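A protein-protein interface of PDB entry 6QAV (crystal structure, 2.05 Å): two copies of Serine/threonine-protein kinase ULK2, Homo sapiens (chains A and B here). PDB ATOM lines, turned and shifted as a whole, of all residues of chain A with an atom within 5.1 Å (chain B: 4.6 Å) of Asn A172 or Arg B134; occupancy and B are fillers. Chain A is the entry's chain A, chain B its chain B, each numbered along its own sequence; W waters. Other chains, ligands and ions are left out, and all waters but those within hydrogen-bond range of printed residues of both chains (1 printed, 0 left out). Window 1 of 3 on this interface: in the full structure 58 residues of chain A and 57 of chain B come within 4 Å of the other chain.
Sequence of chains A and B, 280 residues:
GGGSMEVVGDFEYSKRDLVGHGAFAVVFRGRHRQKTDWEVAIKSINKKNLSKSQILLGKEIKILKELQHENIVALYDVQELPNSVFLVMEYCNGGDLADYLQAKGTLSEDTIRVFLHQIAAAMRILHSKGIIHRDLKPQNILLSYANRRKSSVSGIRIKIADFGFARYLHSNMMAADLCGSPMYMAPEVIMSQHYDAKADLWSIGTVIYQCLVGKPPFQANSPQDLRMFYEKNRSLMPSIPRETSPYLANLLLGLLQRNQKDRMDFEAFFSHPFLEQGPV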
ATOM      1  N   TYR A 168     -15.055 -12.163  27.730  1.00  0.00           N
ATOM      2  CA  TYR A 168     -16.362 -12.036  28.349  1.00  0.00           C
ATOM      3  C   TYR A 168     -17.353 -12.878  27.554  1.00  0.00           C
ATOM      4  O   TYR A 168     -17.501 -12.692  26.343  1.00  0.00           O
ATOM      5  CB  TYR A 168     -16.800 -10.571  28.355  1.00  0.00           C
ATOM      6  CG  TYR A 168     -16.018  -9.671  29.271  1.00  0.00           C
ATOM      7  CD1 TYR A 168     -16.401  -9.502  30.587  1.00  0.00           C
ATOM      8  CD2 TYR A 168     -14.928  -8.944  28.819  1.00  0.00           C
ATOM      9  CE1 TYR A 168     -15.725  -8.645  31.436  1.00  0.00           C
ATOM     10  CE2 TYR A 168     -14.219  -8.105  29.667  1.00  0.00           C
ATOM     11  CZ  TYR A 168     -14.636  -7.945  30.971  1.00  0.00           C
ATOM     12  OH  TYR A 168     -13.936  -7.180  31.837  1.00  0.00           O
ATOM     13  N   LEU A 169     -18.106 -13.719  28.242  1.00  0.00           N
ATOM     14  CA  LEU A 169     -19.154 -14.549  27.584  1.00  0.00           C
ATOM     15  C   LEU A 169     -20.237 -13.649  26.949  1.00  0.00           C
ATOM     16  O   LEU A 169     -20.805 -14.023  25.985  1.00  0.00           O
ATOM     17  CB  LEU A 169     -19.771 -15.499  28.604  1.00  0.00           C
ATOM     18  CG  LEU A 169     -18.842 -16.581  29.191  1.00  0.00           C
ATOM     19  CD1 LEU A 169     -19.597 -17.464  30.175  1.00  0.00           C
ATOM     20  CD2 LEU A 169     -18.220 -17.441  28.118  1.00  0.00           C
ATOM     21  N   HIS A 170     -20.514 -12.467  27.505  1.00  0.00           N
ATOM     22  CA  HIS A 170     -21.640 -11.619  27.055  1.00  0.00           C
ATOM     23  C   HIS A 170     -21.210 -10.619  25.957  1.00  0.00           C
ATOM     24  O   HIS A 170     -22.045  -9.816  25.474  1.00  0.00           O
ATOM     25  CB  HIS A 170     -22.266 -10.928  28.279  1.00  0.00           C
ATOM     26  CG  HIS A 170     -23.378  -9.964  27.982  1.00  0.00           C
ATOM     27  ND1 HIS A 170     -23.134  -8.606  27.691  1.00  0.00           N
ATOM     28  CD2 HIS A 170     -24.728 -10.120  27.972  1.00  0.00           C
ATOM     29  CE1 HIS A 170     -24.287  -7.992  27.499  1.00  0.00           C
ATOM     30  NE2 HIS A 170     -25.280  -8.900  27.665  1.00  0.00           N
ATOM     31  N   SER A 171     -19.942 -10.673  25.500  1.00  0.00           N
ATOM     32  CA  SER A 171     -19.459  -9.656  24.558  1.00  0.00           C
ATOM     33  C   SER A 171     -20.251  -9.699  23.228  1.00  0.00           C
ATOM     34  O   SER A 171     -20.599  -8.633  22.698  1.00  0.00           O
ATOM     35  CB  SER A 171     -17.977  -9.743  24.310  1.00  0.00           C
ATOM     36  OG  SER A 171     -17.655 -10.946  23.645  1.00  0.00           O
ATOM     37  N   ASN A 172     -20.543 -10.901  22.690  1.00  0.00           N
ATOM     38  CA  ASN A 172     -21.284 -10.996  21.415  1.00  0.00           C
ATOM     39  C   ASN A 172     -22.705 -10.440  21.575  1.00  0.00           C
ATOM     40  O   ASN A 172     -23.174  -9.702  20.704  1.00  0.00           O
ATOM     41  CB  ASN A 172     -21.266 -12.402  20.824  1.00  0.00           C
ATOM     42  CG  ASN A 172     -19.925 -12.702  20.169  1.00  0.00           C
ATOM     43  OD1 ASN A 172     -19.226 -11.799  19.712  1.00  0.00           O
ATOM     44  ND2 ASN A 172     -19.558 -13.971  20.113  1.00  0.00           N
ATOM     45  N   MET A 173     -23.359 -10.747  22.695  1.00  0.00           N
ATOM     46  CA  MET A 173     -24.681 -10.201  22.969  1.00  0.00           C
ATOM     47  C   MET A 173     -24.603  -8.675  23.129  1.00  0.00           C
ATOM     48  O   MET A 173     -25.509  -7.976  22.668  1.00  0.00           O
ATOM     49  CB  MET A 173     -25.344 -10.848  24.192  1.00  0.00           C
ATOM     50  CG  MET A 173     -26.391 -11.934  23.825  1.00  0.00           C
ATOM     51  SD  MET A 173     -27.473 -11.574  22.354  1.00  0.00           S
ATOM     52  CE  MET A 173     -28.792 -10.580  23.055  1.00  0.00           C
ATOM     53  N   MET A 174     -23.515  -8.168  23.720  1.00  0.00           N
ATOM     54  CA  MET A 174     -23.320  -6.697  23.844  1.00  0.00           C
ATOM     55  C   MET A 174     -23.114  -6.056  22.450  1.00  0.00           C
ATOM     56  O   MET A 174     -23.680  -5.008  22.157  1.00  0.00           O
ATOM     57  CB  MET A 174     -22.136  -6.344  24.757  1.00  0.00           C
ATOM     58  CG  MET A 174     -22.124  -4.856  25.197  1.00  0.00           C
ATOM     59  SD  MET A 174     -20.505  -4.265  25.870  1.00  0.00           S
ATOM     60  CE  MET A 174     -20.690  -2.480  25.765  1.00  0.00           C
ATOM     61  N   ALA A 175     -22.295  -6.687  21.600  1.00  0.00           N
ATOM     62  CA  ALA A 175     -22.091  -6.233  20.208  1.00  0.00           C
ATOM     63  C   ALA A 175     -23.442  -6.092  19.493  1.00  0.00           C
ATOM     64  O   ALA A 175     -23.682  -5.094  18.840  1.00  0.00           O
ATOM     65  CB  ALA A 175     -21.181  -7.180  19.462  1.00  0.00           C
ATOM     66  N   ALA A 176     -24.303  -7.110  19.617  1.00  0.00           N
ATOM     67  CA  ALA A 176     -25.621  -7.156  18.955  1.00  0.00           C
ATOM     68  C   ALA A 176     -26.497  -5.994  19.438  1.00  0.00           C
ATOM     69  O   ALA A 176     -27.143  -5.323  18.615  1.00  0.00           O
ATOM     70  CB  ALA A 176     -26.292  -8.479  19.214  1.00  0.00           C
ATOM     71  N   MET A 185     -27.381 -11.497  12.049  1.00  0.00           N
ATOM     72  CA  MET A 185     -26.290 -12.166  12.720  1.00  0.00           C
ATOM     73  C   MET A 185     -26.600 -13.666  12.795  1.00  0.00           C
ATOM     74  O   MET A 185     -27.784 -14.046  12.933  1.00  0.00           O
ATOM     75  CB  MET A 185     -26.125 -11.629  14.143  1.00  0.00           C
ATOM     76  CG  MET A 185     -25.276 -10.376  14.237  1.00  0.00           C
ATOM     77  SD  MET A 185     -24.736 -10.073  15.918  1.00  0.00           S
ATOM     78  CE  MET A 185     -23.395  -8.904  15.666  1.00  0.00           C
ATOM     79  N   VAL A 189     -23.641 -17.022  16.660  1.00  0.00           N
ATOM     80  CA  VAL A 189     -22.924 -15.834  17.103  1.00  0.00           C
ATOM     81  C   VAL A 189     -23.691 -15.206  18.285  1.00  0.00           C
ATOM     82  O   VAL A 189     -23.119 -14.939  19.347  1.00  0.00           O
ATOM     83  CB  VAL A 189     -22.735 -14.804  15.966  1.00  0.00           C
ATOM     84  CG1 VAL A 189     -22.048 -13.546  16.488  1.00  0.00           C
ATOM     85  CG2 VAL A 189     -22.002 -15.375  14.763  1.00  0.00           C
ATOM     86  N   SER A 192     -23.354 -17.468  21.566  1.00  0.00           N
ATOM     87  CA  SER A 192     -21.984 -18.058  21.699  1.00  0.00           C
ATOM     88  C   SER A 192     -21.551 -18.168  23.166  1.00  0.00           C
ATOM     89  O   SER A 192     -20.680 -18.958  23.499  1.00  0.00           O
ATOM     90  CB  SER A 192     -20.974 -17.277  20.909  1.00  0.00           C
ATOM     91  OG  SER A 192     -21.026 -15.896  21.244  1.00  0.00           O
ATOM     92  N   ILE B 132     -13.827 -14.528   8.992  1.00  0.00           N
ATOM     93  CA  ILE B 132     -15.245 -14.444   9.033  1.00  0.00           C
ATOM     94  C   ILE B 132     -15.622 -13.028   9.479  1.00  0.00           C
ATOM     95  O   ILE B 132     -15.068 -12.497  10.439  1.00  0.00           O
ATOM     96  CB  ILE B 132     -15.837 -15.520   9.958  1.00  0.00           C
ATOM     97  CG1 ILE B 132     -15.428 -15.323  11.414  1.00  0.00           C
ATOM     98  CG2 ILE B 132     -15.449 -16.891   9.468  1.00  0.00           C
ATOM     99  CD1 ILE B 132     -15.998 -16.341  12.386  1.00  0.00           C
ATOM    100  N   HIS B 133     -16.546 -12.432   8.756  1.00  0.00           N
ATOM    101  CA  HIS B 133     -16.933 -11.036   8.887  1.00  0.00           C
ATOM    102  C   HIS B 133     -17.796 -10.867  10.143  1.00  0.00           C
ATOM    103  O   HIS B 133     -17.548  -9.948  10.972  1.00  0.00           O
ATOM    104  CB  HIS B 133     -17.677 -10.604   7.627  1.00  0.00           C
ATOM    105  CG  HIS B 133     -18.109  -9.173   7.657  1.00  0.00           C
ATOM    106  ND1 HIS B 133     -19.103  -8.724   8.489  1.00  0.00           N
ATOM    107  CD2 HIS B 133     -17.676  -8.103   6.943  1.00  0.00           C
ATOM    108  CE1 HIS B 133     -19.279  -7.436   8.289  1.00  0.00           C
ATOM    109  NE2 HIS B 133     -18.412  -7.029   7.343  1.00  0.00           N
ATOM    110  N   ARG B 134     -18.809 -11.765  10.258  1.00  0.00           N
ATOM    111  CA  ARG B 134     -19.636 -12.005  11.446  1.00  0.00           C
ATOM    112  C   ARG B 134     -20.732 -10.956  11.606  1.00  0.00           C
ATOM    113  O   ARG B 134     -21.595 -11.135  12.458  1.00  0.00           O
ATOM    114  CB  ARG B 134     -18.845 -12.077  12.757  1.00  0.00           C
ATOM    115  CG  ARG B 134     -17.849 -13.233  12.843  1.00  0.00           C
ATOM    116  CD  ARG B 134     -17.611 -13.669  14.280  1.00  0.00           C
ATOM    117  NE  ARG B 134     -17.114 -12.538  15.009  1.00  0.00           N
ATOM    118  CZ  ARG B 134     -17.382 -12.241  16.265  1.00  0.00           C
ATOM    119  NH1 ARG B 134     -17.048 -11.047  16.703  1.00  0.00           N
ATOM    120  NH2 ARG B 134     -17.945 -13.116  17.084  1.00  0.00           N
ATOM    121  N   ASP B 135     -20.737  -9.905  10.777  1.00  0.00           N
ATOM    122  CA  ASP B 135     -21.774  -8.872  10.884  1.00  0.00           C
ATOM    123  C   ASP B 135     -22.240  -8.417   9.502  1.00  0.00           C
ATOM    124  O   ASP B 135     -22.572  -7.256   9.327  1.00  0.00           O
ATOM    125  CB  ASP B 135     -21.278  -7.665  11.681  1.00  0.00           C
ATOM    126  CG  ASP B 135     -22.408  -6.734  12.129  1.00  0.00           C
ATOM    127  OD1 ASP B 135     -23.481  -7.224  12.395  1.00  0.00           O
ATOM    128  OD2 ASP B 135     -22.196  -5.517  12.167  1.00  0.00           O
ATOM    129  N   LEU B 136     -22.319  -9.337   8.539  1.00  0.00           N
ATOM    130  CA  LEU B 136     -22.793  -8.984   7.218  1.00  0.00           C
ATOM    131  C   LEU B 136     -24.260  -8.588   7.304  1.00  0.00           C
ATOM    132  O   LEU B 136     -25.095  -9.314   7.899  1.00  0.00           O
ATOM    133  CB  LEU B 136     -22.674 -10.165   6.267  1.00  0.00           C
ATOM    134  CG  LEU B 136     -21.335 -10.390   5.605  1.00  0.00           C
ATOM    135  CD1 LEU B 136     -21.477 -11.542   4.659  1.00  0.00           C
ATOM    136  CD2 LEU B 136     -20.823  -9.153   4.859  1.00  0.00           C
ATOM    137  N   PHE B 165     -15.911  -6.260  13.500  1.00  0.00           N
ATOM    138  CA  PHE B 165     -16.364  -7.383  14.310  1.00  0.00           C
ATOM    139  C   PHE B 165     -15.784  -8.692  13.741  1.00  0.00           C
ATOM    140  O   PHE B 165     -16.044  -9.798  14.282  1.00  0.00           O
ATOM    141  CB  PHE B 165     -17.896  -7.322  14.373  1.00  0.00           C
ATOM    142  CG  PHE B 165     -18.580  -8.207  15.395  1.00  0.00           C
ATOM    143  CD1 PHE B 165     -18.302  -8.092  16.764  1.00  0.00           C
ATOM    144  CD2 PHE B 165     -19.559  -9.131  14.994  1.00  0.00           C
ATOM    145  CE1 PHE B 165     -18.948  -8.897  17.694  1.00  0.00           C
ATOM    146  CE2 PHE B 165     -20.232  -9.903  15.935  1.00  0.00           C
ATOM    147  CZ  PHE B 165     -19.922  -9.786  17.279  1.00  0.00           C
ATOM    148  N   ARG B 167     -13.283 -11.805  12.614  1.00  0.00           N
ATOM    149  CA  ARG B 167     -12.280 -12.615  13.345  1.00  0.00           C
ATOM    150  C   ARG B 167     -11.590 -13.580  12.379  1.00  0.00           C
ATOM    151  O   ARG B 167     -12.113 -13.933  11.348  1.00  0.00           O
ATOM    152  CB  ARG B 167     -12.941 -13.425  14.474  1.00  0.00           C
ATOM    153  CG  ARG B 167     -13.713 -12.594  15.488  1.00  0.00           C
ATOM    154  CD  ARG B 167     -12.760 -11.833  16.384  1.00  0.00           C
ATOM    155  NE  ARG B 167     -13.436 -11.040  17.411  1.00  0.00           N
ATOM    156  CZ  ARG B 167     -13.671  -9.719  17.309  1.00  0.00           C
ATOM    157  NH1 ARG B 167     -14.378  -9.130  18.251  1.00  0.00           N
ATOM    158  NH2 ARG B 167     -13.236  -9.019  16.260  1.00  0.00           N
ATOM    159  N   ASP B 196     -18.155 -21.115  14.380  1.00  0.00           N
ATOM    160  CA  ASP B 196     -18.805 -19.994  13.694  1.00  0.00           C
ATOM    161  C   ASP B 196     -18.238 -19.863  12.263  1.00  0.00           C
ATOM    162  O   ASP B 196     -18.434 -18.855  11.604  1.00  0.00           O
ATOM    163  CB  ASP B 196     -18.730 -18.710  14.538  1.00  0.00           C
ATOM    164  CG  ASP B 196     -17.327 -18.264  14.924  1.00  0.00           C
ATOM    165  OD1 ASP B 196     -16.381 -19.099  14.750  1.00  0.00           O
ATOM    166  OD2 ASP B 196     -17.183 -17.064  15.383  1.00  0.00           O
ATOM    167  N   ASP B 200     -21.174 -16.288   8.193  1.00  0.00           N
ATOM    168  CA  ASP B 200     -21.417 -15.382   7.078  1.00  0.00           C
ATOM    169  C   ASP B 200     -22.444 -15.999   6.105  1.00  0.00           C
ATOM    170  O   ASP B 200     -23.165 -15.291   5.427  1.00  0.00           O
ATOM    171  CB  ASP B 200     -20.101 -15.022   6.383  1.00  0.00           C
ATOM    172  CG  ASP B 200     -19.214 -14.103   7.218  1.00  0.00           C
ATOM    173  OD1 ASP B 200     -19.748 -13.479   8.177  1.00  0.00           O
ATOM    174  OD2 ASP B 200     -17.993 -14.061   6.953  1.00  0.00           O
HETATM  175  O   HOH W   1     -25.117  -9.489  10.657  1.00  0.00           O
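The side-chain amide oxygen (OD1) of Asn A172 sits at hydrogen-bond distance from the guanidinium group (NH2) of Arg B134 (3.2 Å).
The side-chain amide nitrogen of Asn A172 lies within hydrogen-bond range of the side-chain hydroxyl of Ser A192 (2.7 Å). The guanidinium group (NH1) of Arg B134 lies within hydrogen-bond range of the backbone carbonyl oxygen (O) of Phe B165 (2.9 Å). OD1 of Asp B200 sits at hydrogen-bond distance from N of Arg B134. N of Asp B135 is in hydrogen-bond range of ND1 of His B133, 3.0 Å away.
Among the printed residues, pairs that only touch across the chains: Asn A172 with Phe B165 (3.2 Å), Ala A175 with Phe B165 (3.3 Å), Met A185 with Phe B165 (3.3 Å) and Met A185 with Asp B135 (3.7 Å).
Asn A172 touches just these residues of chain B: Arg B134 and Phe B165. Arg B134 touches just one residue of chain A: Asn A172. Of the printed residues of chain A, Asp B135 touches Met A185 (3.7 Å). Printed residues of chain B within 4 Å of Ala A175: Phe B165. Of the printed residues of chain A, Phe B165 touches Asn A172, Ala A175 and Met A185. Of the printed residues of chain B, Met A185 touches Asp B135 and Phe B165. The nearest printed residue of chain B that does not touch Asn A172 is Arg B167 (5.7 Å). The nearest printed residue of chain A that does not touch Arg B134 is Met A185 (4.2 Å). The nearest printed residue of chain A that does not touch Phe B165 is Val A189 (4.1 Å).
Of the 9 printed residues of chain B, 3 touch a printed residue of chain A. Hydrophobic or aromatic side chains of chain B that line the printed part of chain A: Phe B165. Hydrophobic or aromatic side chains of chain A that line the printed part of chain B: Ala A175 and Met A185.
No position is printed for both chains.
Water W1 lies within hydrogen-bond range of O of Leu B136, OD1 of Asp B135 and N of Met A185.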
